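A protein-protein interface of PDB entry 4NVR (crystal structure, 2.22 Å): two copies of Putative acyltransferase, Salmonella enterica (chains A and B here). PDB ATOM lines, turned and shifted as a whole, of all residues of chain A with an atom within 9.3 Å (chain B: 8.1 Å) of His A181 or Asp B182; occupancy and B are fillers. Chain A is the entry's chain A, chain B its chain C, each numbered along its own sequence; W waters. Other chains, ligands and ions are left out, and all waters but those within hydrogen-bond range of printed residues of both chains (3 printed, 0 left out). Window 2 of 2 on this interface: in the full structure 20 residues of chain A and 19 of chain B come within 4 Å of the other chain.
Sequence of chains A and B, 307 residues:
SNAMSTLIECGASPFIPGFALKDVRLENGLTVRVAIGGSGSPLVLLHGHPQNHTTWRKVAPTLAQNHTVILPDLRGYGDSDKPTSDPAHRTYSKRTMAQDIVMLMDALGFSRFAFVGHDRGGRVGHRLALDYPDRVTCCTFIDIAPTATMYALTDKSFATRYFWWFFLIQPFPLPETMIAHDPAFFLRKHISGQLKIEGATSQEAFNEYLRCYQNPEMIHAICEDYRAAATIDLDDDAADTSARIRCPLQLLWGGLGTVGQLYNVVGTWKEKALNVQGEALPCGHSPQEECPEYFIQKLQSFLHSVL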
ATOM      1  N   PHE A 167      22.515  17.582  21.792  1.00  0.00           N
ATOM      2  CA  PHE A 167      21.904  16.432  22.445  1.00  0.00           C
ATOM      3  C   PHE A 167      22.258  15.129  21.716  1.00  0.00           C
ATOM      4  O   PHE A 167      22.597  14.122  22.333  1.00  0.00           O
ATOM      5  CB  PHE A 167      20.396  16.620  22.468  1.00  0.00           C
ATOM      6  CG  PHE A 167      19.660  15.543  23.202  1.00  0.00           C
ATOM      7  CD1 PHE A 167      19.501  15.608  24.566  1.00  0.00           C
ATOM      8  CD2 PHE A 167      19.101  14.490  22.511  1.00  0.00           C
ATOM      9  CE1 PHE A 167      18.811  14.613  25.246  1.00  0.00           C
ATOM     10  CE2 PHE A 167      18.409  13.498  23.162  1.00  0.00           C
ATOM     11  CZ  PHE A 167      18.267  13.550  24.531  1.00  0.00           C
ATOM     12  N   PRO A 173      25.067   5.568  25.461  1.00  0.00           N
ATOM     13  CA  PRO A 173      23.865   5.394  24.662  1.00  0.00           C
ATOM     14  C   PRO A 173      22.779   6.349  25.040  1.00  0.00           C
ATOM     15  O   PRO A 173      21.605   5.996  24.965  1.00  0.00           O
ATOM     16  CB  PRO A 173      23.401   4.001  25.087  1.00  0.00           C
ATOM     17  CG  PRO A 173      23.691   4.003  26.571  1.00  0.00           C
ATOM     18  CD  PRO A 173      24.921   4.894  26.767  1.00  0.00           C
ATOM     19  N   LEU A 174      23.141   7.554  25.425  1.00  0.00           N
ATOM     20  CA  LEU A 174      22.146   8.487  25.933  1.00  0.00           C
ATOM     21  C   LEU A 174      21.075   8.908  24.927  1.00  0.00           C
ATOM     22  O   LEU A 174      19.889   8.686  25.153  1.00  0.00           O
ATOM     23  CB  LEU A 174      22.851   9.684  26.589  1.00  0.00           C
ATOM     24  CG  LEU A 174      22.010  10.914  26.843  1.00  0.00           C
ATOM     25  CD1 LEU A 174      20.674  10.573  27.465  1.00  0.00           C
ATOM     26  CD2 LEU A 174      22.810  11.853  27.731  1.00  0.00           C
ATOM     27  N   PRO A 175      21.481   9.508  23.817  1.00  0.00           N
ATOM     28  CA  PRO A 175      20.455   9.901  22.868  1.00  0.00           C
ATOM     29  C   PRO A 175      19.747   8.688  22.275  1.00  0.00           C
ATOM     30  O   PRO A 175      18.508   8.717  22.066  1.00  0.00           O
ATOM     31  CB  PRO A 175      21.232  10.695  21.813  1.00  0.00           C
ATOM     32  CG  PRO A 175      22.638  10.235  21.941  1.00  0.00           C
ATOM     33  CD  PRO A 175      22.846   9.781  23.337  1.00  0.00           C
ATOM     34  N   GLU A 176      20.498   7.613  22.048  1.00  0.00           N
ATOM     35  CA  GLU A 176      19.879   6.404  21.506  1.00  0.00           C
ATOM     36  C   GLU A 176      18.822   5.916  22.490  1.00  0.00           C
ATOM     37  O   GLU A 176      17.783   5.426  22.093  1.00  0.00           O
ATOM     38  CB  GLU A 176      20.876   5.263  21.266  1.00  0.00           C
ATOM     39  CG  GLU A 176      21.861   5.461  20.120  1.00  0.00           C
ATOM     40  CD  GLU A 176      23.131   6.195  20.489  1.00  0.00           C
ATOM     41  OE1 GLU A 176      23.199   6.862  21.556  1.00  0.00           O
ATOM     42  OE2 GLU A 176      24.101   6.065  19.700  1.00  0.00           O
ATOM     43  N   THR A 177      19.076   6.063  23.780  1.00  0.00           N
ATOM     44  CA  THR A 177      18.084   5.548  24.723  1.00  0.00           C
ATOM     45  C   THR A 177      16.879   6.463  24.781  1.00  0.00           C
ATOM     46  O   THR A 177      15.759   6.002  24.856  1.00  0.00           O
ATOM     47  CB  THR A 177      18.678   5.328  26.107  1.00  0.00           C
ATOM     48  OG1 THR A 177      19.815   4.473  25.995  1.00  0.00           O
ATOM     49  CG2 THR A 177      17.660   4.697  27.036  1.00  0.00           C
ATOM     50  N   MET A 178      17.102   7.763  24.713  1.00  0.00           N
ATOM     51  CA  MET A 178      15.975   8.695  24.796  1.00  0.00           C
ATOM     52  C   MET A 178      15.030   8.547  23.635  1.00  0.00           C
ATOM     53  O   MET A 178      13.822   8.440  23.836  1.00  0.00           O
ATOM     54  CB  MET A 178      16.446  10.133  24.840  1.00  0.00           C
ATOM     55  CG  MET A 178      17.474  10.276  25.935  1.00  0.00           C
ATOM     56  SD  MET A 178      16.614  10.778  27.609  1.00  0.00           S
ATOM     57  CE  MET A 178      17.151  12.643  27.424  1.00  0.00           C
ATOM     58  N   ILE A 179      15.568   8.574  22.413  1.00  0.00           N
ATOM     59  CA  ILE A 179      14.755   8.431  21.220  1.00  0.00           C
ATOM     60  C   ILE A 179      13.967   7.128  21.251  1.00  0.00           C
ATOM     61  O   ILE A 179      12.785   7.103  20.915  1.00  0.00           O
ATOM     62  CB  ILE A 179      15.629   8.507  19.951  1.00  0.00           C
ATOM     63  CG1 ILE A 179      16.181   9.934  19.821  1.00  0.00           C
ATOM     64  CG2 ILE A 179      14.823   8.120  18.694  1.00  0.00           C
ATOM     65  CD1 ILE A 179      17.414  10.050  18.990  1.00  0.00           C
ATOM     66  N   ALA A 180      14.613   6.045  21.653  1.00  0.00           N
ATOM     67  CA  ALA A 180      13.943   4.737  21.671  1.00  0.00           C
ATOM     68  C   ALA A 180      12.723   4.726  22.577  1.00  0.00           C
ATOM     69  O   ALA A 180      11.882   3.892  22.417  1.00  0.00           O
ATOM     70  CB  ALA A 180      14.900   3.651  22.107  1.00  0.00           C
ATOM     71  N   HIS A 181      12.626   5.649  23.527  1.00  0.00           N
ATOM     72  CA  HIS A 181      11.449   5.662  24.419  1.00  0.00           C
ATOM     73  C   HIS A 181      10.188   5.853  23.639  1.00  0.00           C
ATOM     74  O   HIS A 181       9.149   5.353  24.049  1.00  0.00           O
ATOM     75  CB  HIS A 181      11.486   6.808  25.451  1.00  0.00           C
ATOM     76  CG  HIS A 181      12.568   6.686  26.466  1.00  0.00           C
ATOM     77  ND1 HIS A 181      13.353   7.753  26.850  1.00  0.00           N
ATOM     78  CD2 HIS A 181      12.983   5.627  27.197  1.00  0.00           C
ATOM     79  CE1 HIS A 181      14.204   7.358  27.779  1.00  0.00           C
ATOM     80  NE2 HIS A 181      13.997   6.072  28.012  1.00  0.00           N
ATOM     81  N   ASP A 182      10.265   6.644  22.560  1.00  0.00           N
ATOM     82  CA  ASP A 182       9.087   6.919  21.716  1.00  0.00           C
ATOM     83  C   ASP A 182       9.547   7.464  20.359  1.00  0.00           C
ATOM     84  O   ASP A 182       9.546   8.675  20.099  1.00  0.00           O
ATOM     85  CB  ASP A 182       8.113   7.887  22.408  1.00  0.00           C
ATOM     86  CG  ASP A 182       6.743   7.932  21.723  1.00  0.00           C
ATOM     87  OD1 ASP A 182       6.555   7.253  20.710  1.00  0.00           O
ATOM     88  OD2 ASP A 182       5.821   8.620  22.221  1.00  0.00           O
ATOM     89  N   PRO A 183       9.927   6.559  19.464  1.00  0.00           N
ATOM     90  CA  PRO A 183      10.431   7.009  18.170  1.00  0.00           C
ATOM     91  C   PRO A 183       9.466   7.920  17.410  1.00  0.00           C
ATOM     92  O   PRO A 183       9.883   8.946  16.904  1.00  0.00           O
ATOM     93  CB  PRO A 183      10.674   5.703  17.422  1.00  0.00           C
ATOM     94  CG  PRO A 183      10.887   4.695  18.510  1.00  0.00           C
ATOM     95  CD  PRO A 183       9.905   5.095  19.556  1.00  0.00           C
ATOM     96  N   ALA A 184       8.186   7.577  17.345  1.00  0.00           N
ATOM     97  CA  ALA A 184       7.247   8.416  16.578  1.00  0.00           C
ATOM     98  C   ALA A 184       7.203   9.847  17.103  1.00  0.00           C
ATOM     99  O   ALA A 184       7.117  10.791  16.323  1.00  0.00           O
ATOM    100  CB  ALA A 184       5.857   7.817  16.559  1.00  0.00           C
ATOM    101  N   PHE A 185       7.237   9.998  18.428  1.00  0.00           N
ATOM    102  CA  PHE A 185       7.255  11.327  19.037  1.00  0.00           C
ATOM    103  C   PHE A 185       8.470  12.106  18.545  1.00  0.00           C
ATOM    104  O   PHE A 185       8.309  13.209  18.053  1.00  0.00           O
ATOM    105  CB  PHE A 185       7.239  11.250  20.568  1.00  0.00           C
ATOM    106  CG  PHE A 185       7.454  12.574  21.241  1.00  0.00           C
ATOM    107  CD1 PHE A 185       6.387  13.428  21.476  1.00  0.00           C
ATOM    108  CD2 PHE A 185       8.725  12.965  21.644  1.00  0.00           C
ATOM    109  CE1 PHE A 185       6.574  14.645  22.109  1.00  0.00           C
ATOM    110  CE2 PHE A 185       8.921  14.190  22.288  1.00  0.00           C
ATOM    111  CZ  PHE A 185       7.842  15.025  22.516  1.00  0.00           C
ATOM    112  N   PHE A 186       9.677  11.542  18.647  1.00  0.00           N
ATOM    113  CA  PHE A 186      10.867  12.258  18.150  1.00  0.00           C
ATOM    114  C   PHE A 186      10.800  12.564  16.661  1.00  0.00           C
ATOM    115  O   PHE A 186      11.236  13.651  16.226  1.00  0.00           O
ATOM    116  CB  PHE A 186      12.172  11.532  18.497  1.00  0.00           C
ATOM    117  CG  PHE A 186      12.525  11.673  19.921  1.00  0.00           C
ATOM    118  CD1 PHE A 186      11.926  10.833  20.887  1.00  0.00           C
ATOM    119  CD2 PHE A 186      13.368  12.697  20.340  1.00  0.00           C
ATOM    120  CE1 PHE A 186      12.185  10.997  22.230  1.00  0.00           C
ATOM    121  CE2 PHE A 186      13.640  12.856  21.695  1.00  0.00           C
ATOM    122  CZ  PHE A 186      13.037  12.008  22.640  1.00  0.00           C
ATOM    123  N   TYR A 213      12.744   4.609  10.878  1.00  0.00           N
ATOM    124  CA  TYR A 213      13.218   5.242  12.124  1.00  0.00           C
ATOM    125  C   TYR A 213      13.055   4.366  13.359  1.00  0.00           C
ATOM    126  O   TYR A 213      13.713   4.602  14.347  1.00  0.00           O
ATOM    127  CB  TYR A 213      12.468   6.563  12.313  1.00  0.00           C
ATOM    128  CG  TYR A 213      13.066   7.578  13.258  1.00  0.00           C
ATOM    129  CD1 TYR A 213      14.200   8.290  12.923  1.00  0.00           C
ATOM    130  CD2 TYR A 213      12.433   7.895  14.444  1.00  0.00           C
ATOM    131  CE1 TYR A 213      14.728   9.254  13.780  1.00  0.00           C
ATOM    132  CE2 TYR A 213      12.946   8.851  15.301  1.00  0.00           C
ATOM    133  CZ  TYR A 213      14.090   9.530  14.962  1.00  0.00           C
ATOM    134  OH  TYR A 213      14.571  10.489  15.842  1.00  0.00           O
ATOM    135  N   ILE A 219      18.684   4.504  14.444  1.00  0.00           N
ATOM    136  CA  ILE A 219      18.767   5.460  15.552  1.00  0.00           C
ATOM    137  C   ILE A 219      20.219   5.699  15.924  1.00  0.00           C
ATOM    138  O   ILE A 219      20.655   6.843  16.042  1.00  0.00           O
ATOM    139  CB  ILE A 219      17.966   4.995  16.783  1.00  0.00           C
ATOM    140  CG1 ILE A 219      16.487   4.828  16.417  1.00  0.00           C
ATOM    141  CG2 ILE A 219      18.107   5.996  17.917  1.00  0.00           C
ATOM    142  CD1 ILE A 219      15.640   4.248  17.533  1.00  0.00           C
ATOM    143  N   GLU B 176       9.666  18.054  29.493  1.00  0.00           N
ATOM    144  CA  GLU B 176       8.814  17.351  30.440  1.00  0.00           C
ATOM    145  C   GLU B 176       8.367  15.985  29.905  1.00  0.00           C
ATOM    146  O   GLU B 176       8.374  14.983  30.643  1.00  0.00           O
ATOM    147  CB  GLU B 176       7.585  18.190  30.789  1.00  0.00           C
ATOM    148  CG  GLU B 176       7.857  19.465  31.597  1.00  0.00           C
ATOM    149  CD  GLU B 176       8.046  20.725  30.765  1.00  0.00           C
ATOM    150  OE1 GLU B 176       8.310  20.676  29.512  1.00  0.00           O
ATOM    151  OE2 GLU B 176       7.918  21.800  31.385  1.00  0.00           O
ATOM    152  N   THR B 177       7.997  15.943  28.633  1.00  0.00           N
ATOM    153  CA  THR B 177       7.544  14.704  28.022  1.00  0.00           C
ATOM    154  C   THR B 177       8.689  13.729  27.961  1.00  0.00           C
ATOM    155  O   THR B 177       8.538  12.566  28.247  1.00  0.00           O
ATOM    156  CB  THR B 177       7.023  14.955  26.601  1.00  0.00           C
ATOM    157  OG1 THR B 177       6.001  15.944  26.660  1.00  0.00           O
ATOM    158  CG2 THR B 177       6.459  13.686  25.973  1.00  0.00           C
ATOM    159  N   MET B 178       9.856  14.220  27.605  1.00  0.00           N
ATOM    160  CA  MET B 178      11.008  13.343  27.483  1.00  0.00           C
ATOM    161  C   MET B 178      11.457  12.783  28.821  1.00  0.00           C
ATOM    162  O   MET B 178      11.770  11.594  28.934  1.00  0.00           O
ATOM    163  CB  MET B 178      12.111  14.101  26.753  1.00  0.00           C
ATOM    164  CG  MET B 178      11.783  14.111  25.257  1.00  0.00           C
ATOM    165  SD  MET B 178      13.125  15.150  24.241  1.00  0.00           S
ATOM    166  CE  MET B 178      14.733  14.121  24.757  1.00  0.00           C
ATOM    167  N   ILE B 179      11.519  13.625  29.848  1.00  0.00           N
ATOM    168  CA  ILE B 179      11.932  13.139  31.141  1.00  0.00           C
ATOM    169  C   ILE B 179      10.911  12.100  31.636  1.00  0.00           C
ATOM    170  O   ILE B 179      11.302  11.044  32.138  1.00  0.00           O
ATOM    171  CB  ILE B 179      12.144  14.306  32.125  1.00  0.00           C
ATOM    172  CG1 ILE B 179      13.363  15.134  31.679  1.00  0.00           C
ATOM    173  CG2 ILE B 179      12.347  13.784  33.539  1.00  0.00           C
ATOM    174  CD1 ILE B 179      13.463  16.489  32.344  1.00  0.00           C
ATOM    175  N   ALA B 180       9.617  12.387  31.463  1.00  0.00           N
ATOM    176  CA  ALA B 180       8.528  11.472  31.856  1.00  0.00           C
ATOM    177  C   ALA B 180       8.626  10.070  31.258  1.00  0.00           C
ATOM    178  O   ALA B 180       8.108   9.127  31.835  1.00  0.00           O
ATOM    179  CB  ALA B 180       7.170  12.062  31.472  1.00  0.00           C
ATOM    180  N   HIS B 181       9.250   9.921  30.090  1.00  0.00           N
ATOM    181  CA  HIS B 181       9.397   8.581  29.533  1.00  0.00           C
ATOM    182  C   HIS B 181      10.125   7.637  30.506  1.00  0.00           C
ATOM    183  O   HIS B 181       9.824   6.459  30.565  1.00  0.00           O
ATOM    184  CB  HIS B 181      10.160   8.593  28.207  1.00  0.00           C
ATOM    185  CG  HIS B 181       9.424   9.234  27.081  1.00  0.00           C
ATOM    186  ND1 HIS B 181      10.045  10.074  26.176  1.00  0.00           N
ATOM    187  CD2 HIS B 181       8.125   9.163  26.706  1.00  0.00           C
ATOM    188  CE1 HIS B 181       9.159  10.472  25.278  1.00  0.00           C
ATOM    189  NE2 HIS B 181       7.984   9.947  25.586  1.00  0.00           N
ATOM    190  N   ASP B 182      11.117   8.158  31.221  1.00  0.00           N
ATOM    191  CA  ASP B 182      11.863   7.382  32.211  1.00  0.00           C
ATOM    192  C   ASP B 182      12.578   8.345  33.163  1.00  0.00           C
ATOM    193  O   ASP B 182      13.760   8.688  32.959  1.00  0.00           O
ATOM    194  CB  ASP B 182      12.863   6.460  31.542  1.00  0.00           C
ATOM    195  CG  ASP B 182      13.438   5.427  32.496  1.00  0.00           C
ATOM    196  OD1 ASP B 182      13.554   5.698  33.707  1.00  0.00           O
ATOM    197  OD2 ASP B 182      13.767   4.328  32.032  1.00  0.00           O
ATOM    198  N   PRO B 183      11.866   8.799  34.207  1.00  0.00           N
ATOM    199  CA  PRO B 183      12.502   9.738  35.119  1.00  0.00           C
ATOM    200  C   PRO B 183      13.770   9.211  35.742  1.00  0.00           C
ATOM    201  O   PRO B 183      14.729   9.958  35.866  1.00  0.00           O
ATOM    202  CB  PRO B 183      11.419   9.978  36.178  1.00  0.00           C
ATOM    203  CG  PRO B 183      10.165   9.884  35.401  1.00  0.00           C
ATOM    204  CD  PRO B 183      10.408   8.756  34.408  1.00  0.00           C
ATOM    205  N   ALA B 184      13.795   7.933  36.107  1.00  0.00           N
ATOM    206  CA  ALA B 184      14.968   7.372  36.797  1.00  0.00           C
ATOM    207  C   ALA B 184      16.224   7.337  35.927  1.00  0.00           C
ATOM    208  O   ALA B 184      17.352   7.491  36.399  1.00  0.00           O
ATOM    209  CB  ALA B 184      14.640   5.977  37.319  1.00  0.00           C
ATOM    210  N   PHE B 185      16.022   7.089  34.645  1.00  0.00           N
ATOM    211  CA  PHE B 185      17.118   7.091  33.710  1.00  0.00           C
ATOM    212  C   PHE B 185      17.742   8.494  33.632  1.00  0.00           C
ATOM    213  O   PHE B 185      18.950   8.654  33.738  1.00  0.00           O
ATOM    214  CB  PHE B 185      16.617   6.677  32.333  1.00  0.00           C
ATOM    215  CG  PHE B 185      17.634   6.840  31.262  1.00  0.00           C
ATOM    216  CD1 PHE B 185      18.648   5.908  31.114  1.00  0.00           C
ATOM    217  CD2 PHE B 185      17.597   7.940  30.415  1.00  0.00           C
ATOM    218  CE1 PHE B 185      19.600   6.053  30.144  1.00  0.00           C
ATOM    219  CE2 PHE B 185      18.554   8.083  29.426  1.00  0.00           C
ATOM    220  CZ  PHE B 185      19.554   7.133  29.291  1.00  0.00           C
ATOM    221  N   PHE B 186      16.908   9.504  33.477  1.00  0.00           N
ATOM    222  CA  PHE B 186      17.409  10.840  33.319  1.00  0.00           C
ATOM    223  C   PHE B 186      17.980  11.363  34.663  1.00  0.00           C
ATOM    224  O   PHE B 186      18.960  12.088  34.699  1.00  0.00           O
ATOM    225  CB  PHE B 186      16.318  11.721  32.695  1.00  0.00           C
ATOM    226  CG  PHE B 186      16.850  12.927  32.024  1.00  0.00           C
ATOM    227  CD1 PHE B 186      17.479  12.824  30.791  1.00  0.00           C
ATOM    228  CD2 PHE B 186      16.755  14.167  32.619  1.00  0.00           C
ATOM    229  CE1 PHE B 186      17.995  13.952  30.163  1.00  0.00           C
ATOM    230  CE2 PHE B 186      17.265  15.296  31.996  1.00  0.00           C
ATOM    231  CZ  PHE B 186      17.887  15.184  30.768  1.00  0.00           C
ATOM    232  N   LEU B 187      17.412  10.952  35.778  1.00  0.00           N
ATOM    233  CA  LEU B 187      18.022  11.337  37.046  1.00  0.00           C
ATOM    234  C   LEU B 187      19.448  10.755  37.105  1.00  0.00           C
ATOM    235  O   LEU B 187      20.410  11.468  37.335  1.00  0.00           O
ATOM    236  CB  LEU B 187      17.198  10.823  38.232  1.00  0.00           C
ATOM    237  CG  LEU B 187      17.602  11.284  39.619  1.00  0.00           C
ATOM    238  CD1 LEU B 187      17.605  12.805  39.705  1.00  0.00           C
ATOM    239  CD2 LEU B 187      16.668  10.694  40.667  1.00  0.00           C
ATOM    240  N   ARG B 188      19.561   9.455  36.887  1.00  0.00           N
ATOM    241  CA  ARG B 188      20.847   8.760  36.932  1.00  0.00           C
ATOM    242  C   ARG B 188      21.923   9.448  36.068  1.00  0.00           C
ATOM    243  O   ARG B 188      23.058   9.593  36.509  1.00  0.00           O
ATOM    244  CB  ARG B 188      20.646   7.308  36.486  1.00  0.00           C
ATOM    245  CG  ARG B 188      21.906   6.454  36.354  1.00  0.00           C
ATOM    246  CD  ARG B 188      22.160   5.573  37.554  1.00  0.00           C
ATOM    247  NE  ARG B 188      22.583   6.299  38.740  1.00  0.00           N
ATOM    248  CZ  ARG B 188      22.653   5.756  39.951  1.00  0.00           C
ATOM    249  NH1 ARG B 188      23.056   6.487  40.978  1.00  0.00           N
ATOM    250  NH2 ARG B 188      22.298   4.482  40.143  1.00  0.00           N
ATOM    251  N   LYS B 189      21.574   9.863  34.849  1.00  0.00           N
ATOM    252  CA  LYS B 189      22.558  10.512  33.968  1.00  0.00           C
ATOM    253  C   LYS B 189      23.015  11.824  34.577  1.00  0.00           C
ATOM    254  O   LYS B 189      24.191  12.137  34.533  1.00  0.00           O
ATOM    255  CB  LYS B 189      22.003  10.721  32.568  1.00  0.00           C
ATOM    256  CG  LYS B 189      21.634   9.417  31.859  1.00  0.00           C
ATOM    257  CD  LYS B 189      22.818   8.474  31.584  1.00  0.00           C
ATOM    258  CE  LYS B 189      23.802   9.066  30.587  1.00  0.00           C
ATOM    259  NZ  LYS B 189      24.831   8.080  30.135  1.00  0.00           N
ATOM    260  N   LEU B 210      14.980  10.196  43.826  1.00  0.00           N
ATOM    261  CA  LEU B 210      14.055   9.714  42.775  1.00  0.00           C
ATOM    262  C   LEU B 210      12.600   9.850  43.269  1.00  0.00           C
ATOM    263  O   LEU B 210      11.743  10.242  42.514  1.00  0.00           O
ATOM    264  CB  LEU B 210      14.412   8.295  42.327  1.00  0.00           C
ATOM    265  CG  LEU B 210      13.555   7.677  41.210  1.00  0.00           C
ATOM    266  CD1 LEU B 210      13.562   8.515  39.948  1.00  0.00           C
ATOM    267  CD2 LEU B 210      14.036   6.268  40.891  1.00  0.00           C
ATOM    268  N   TYR B 213      11.765  13.368  42.306  1.00  0.00           N
ATOM    269  CA  TYR B 213      11.953  13.678  40.894  1.00  0.00           C
ATOM    270  C   TYR B 213      10.898  13.031  40.005  1.00  0.00           C
ATOM    271  O   TYR B 213      10.560  13.589  38.953  1.00  0.00           O
ATOM    272  CB  TYR B 213      13.360  13.236  40.485  1.00  0.00           C
ATOM    273  CG  TYR B 213      13.843  13.677  39.139  1.00  0.00           C
ATOM    274  CD1 TYR B 213      14.457  14.919  38.973  1.00  0.00           C
ATOM    275  CD2 TYR B 213      13.759  12.832  38.046  1.00  0.00           C
ATOM    276  CE1 TYR B 213      14.924  15.323  37.734  1.00  0.00           C
ATOM    277  CE2 TYR B 213      14.231  13.208  36.813  1.00  0.00           C
ATOM    278  CZ  TYR B 213      14.812  14.456  36.657  1.00  0.00           C
ATOM    279  OH  TYR B 213      15.287  14.825  35.432  1.00  0.00           O
ATOM    280  N   GLN B 214      10.342  11.894  40.415  1.00  0.00           N
ATOM    281  CA  GLN B 214       9.357  11.237  39.544  1.00  0.00           C
ATOM    282  C   GLN B 214       7.978  11.918  39.548  1.00  0.00           C
ATOM    283  O   GLN B 214       7.151  11.634  38.706  1.00  0.00           O
ATOM    284  CB  GLN B 214       9.303   9.733  39.794  1.00  0.00           C
ATOM    285  CG  GLN B 214       8.801   9.307  41.151  1.00  0.00           C
ATOM    286  CD  GLN B 214       9.101   7.854  41.433  1.00  0.00           C
ATOM    287  OE1 GLN B 214      10.001   7.260  40.833  1.00  0.00           O
ATOM    288  NE2 GLN B 214       8.369   7.277  42.362  1.00  0.00           N
HETATM  289  O   HOH W   1      12.930  10.250  26.194  1.00  0.00           O
HETATM  290  O   HOH W   2      15.266   4.232  29.747  1.00  0.00           O
HETATM  291  O   HOH W   3       5.990  10.459  24.053  1.00  0.00           O
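OD1 of Asp B182 lies close to N of Ala B184 (3.3 Å).
The backbone carbonyl oxygen of Met A178 sits at hydrogen-bond distance from a ring nitrogen (ND1) of His A181.
The side-chain carboxylate (OD1) of Asp B182 is in hydrogen-bond range of the backbone NH (N) of Phe B185.
O of Pro A173 is in hydrogen-bond range of OG1 of Thr A177, at 2.6 Å.
Among the printed residues, merely in contact across the chains: Met A178 with Phe B186, Phe A186 with Met B178, His A181 with His B181, Phe A167 with Met B178, His A181 with Asp B182, Thr A177 with Phe B185, Met A178 with Phe B185, Asp A182 with His B181, Leu A174 with Phe B185, Met A178 with Met B178 and Phe A185 with Thr B177.
Of chain B, only His B181 and Asp B182 come within 4 Å of His A181.
Of chain A, only His A181 (3.7 Å) comes within 4 Å of Asp B182.
No residue of chain B comes within 4 Å of Ala A180.
Of chain A, only His A181 and Asp A182 come within 4 Å of His B181.
No residue of chain A comes within 4 Å of Ala B184.
Printed residues of chain A within 4 Å of Met B178: Phe A167, Met A178 and Phe A186.
Of the printed residues of chain B, Leu A174 touches Phe B185 (3.8 Å).
Of the printed residues of chain A, Phe B186 touches Met A178 (3.2 Å).
Glu B176 touches none of the printed residues of chain A.
The nearest residue of chain B that does not touch His A181 is Phe B185 (4.3 Å).
The nearest residue of chain A that does not touch Asp B182 is Thr A177 (6.3 Å).
The nearest printed residue of chain B that does not touch Phe A167 is Phe B186 (5.0 Å).
Of the 17 printed residues of chain A, 8 touch a printed residue of chain B.
Hydrophobic or aromatic side chains of chain A within 4 Å of the printed part of chain B: Phe A167, Leu A174, Met A178, His A181, Phe A185 and Phe A186.
Printed residues of chain B that touch a printed residue of chain A: Thr B177, Met B178, His B181, Asp B182, Phe B185 and Phe B186.
Hydrophobic or aromatic side chains of chain B within 4 Å of the printed part of chain A: Met B178, His B181, Phe B185 and Phe B186.
Among the printed residues, 11 pairs touch across the chains.
Among the printed residues, no Asp or Glu carboxylate lies within 4 Å of a Lys or Arg side-chain nitrogen of the other chain.
Thr A177 touches Phe B185, and with the chains exchanged Phe A185 touches Thr B177.
Met A178 touches Phe B185, but with the chains exchanged Phe A185 does not touch Met B178 (4.1 Å).
Met A178 touches Phe B186, and with the chains exchanged Phe A186 touches Met B178.
His A181 touches its own counterpart, His B181.
12 positions are printed for both chains.
Of the 11 pairs that touch across the chains among the printed residues, 8 have their exchanged pair printed and touching as well.
Water W3 lies within hydrogen-bond range of a ring nitrogen (NE2) of His B181 and the side-chain carboxylate of Asp A182.
Water W1 lies within hydrogen-bond range of a ring nitrogen (ND1) of His A181, a ring nitrogen (ND1) of His B181, the backbone carbonyl oxygen of Met A178 and the backbone carbonyl oxygen of Met B178.
Water W2 bridges OD2 of Asp B182 (2.7 Å) and NE2 of His A181 (2.8 Å).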
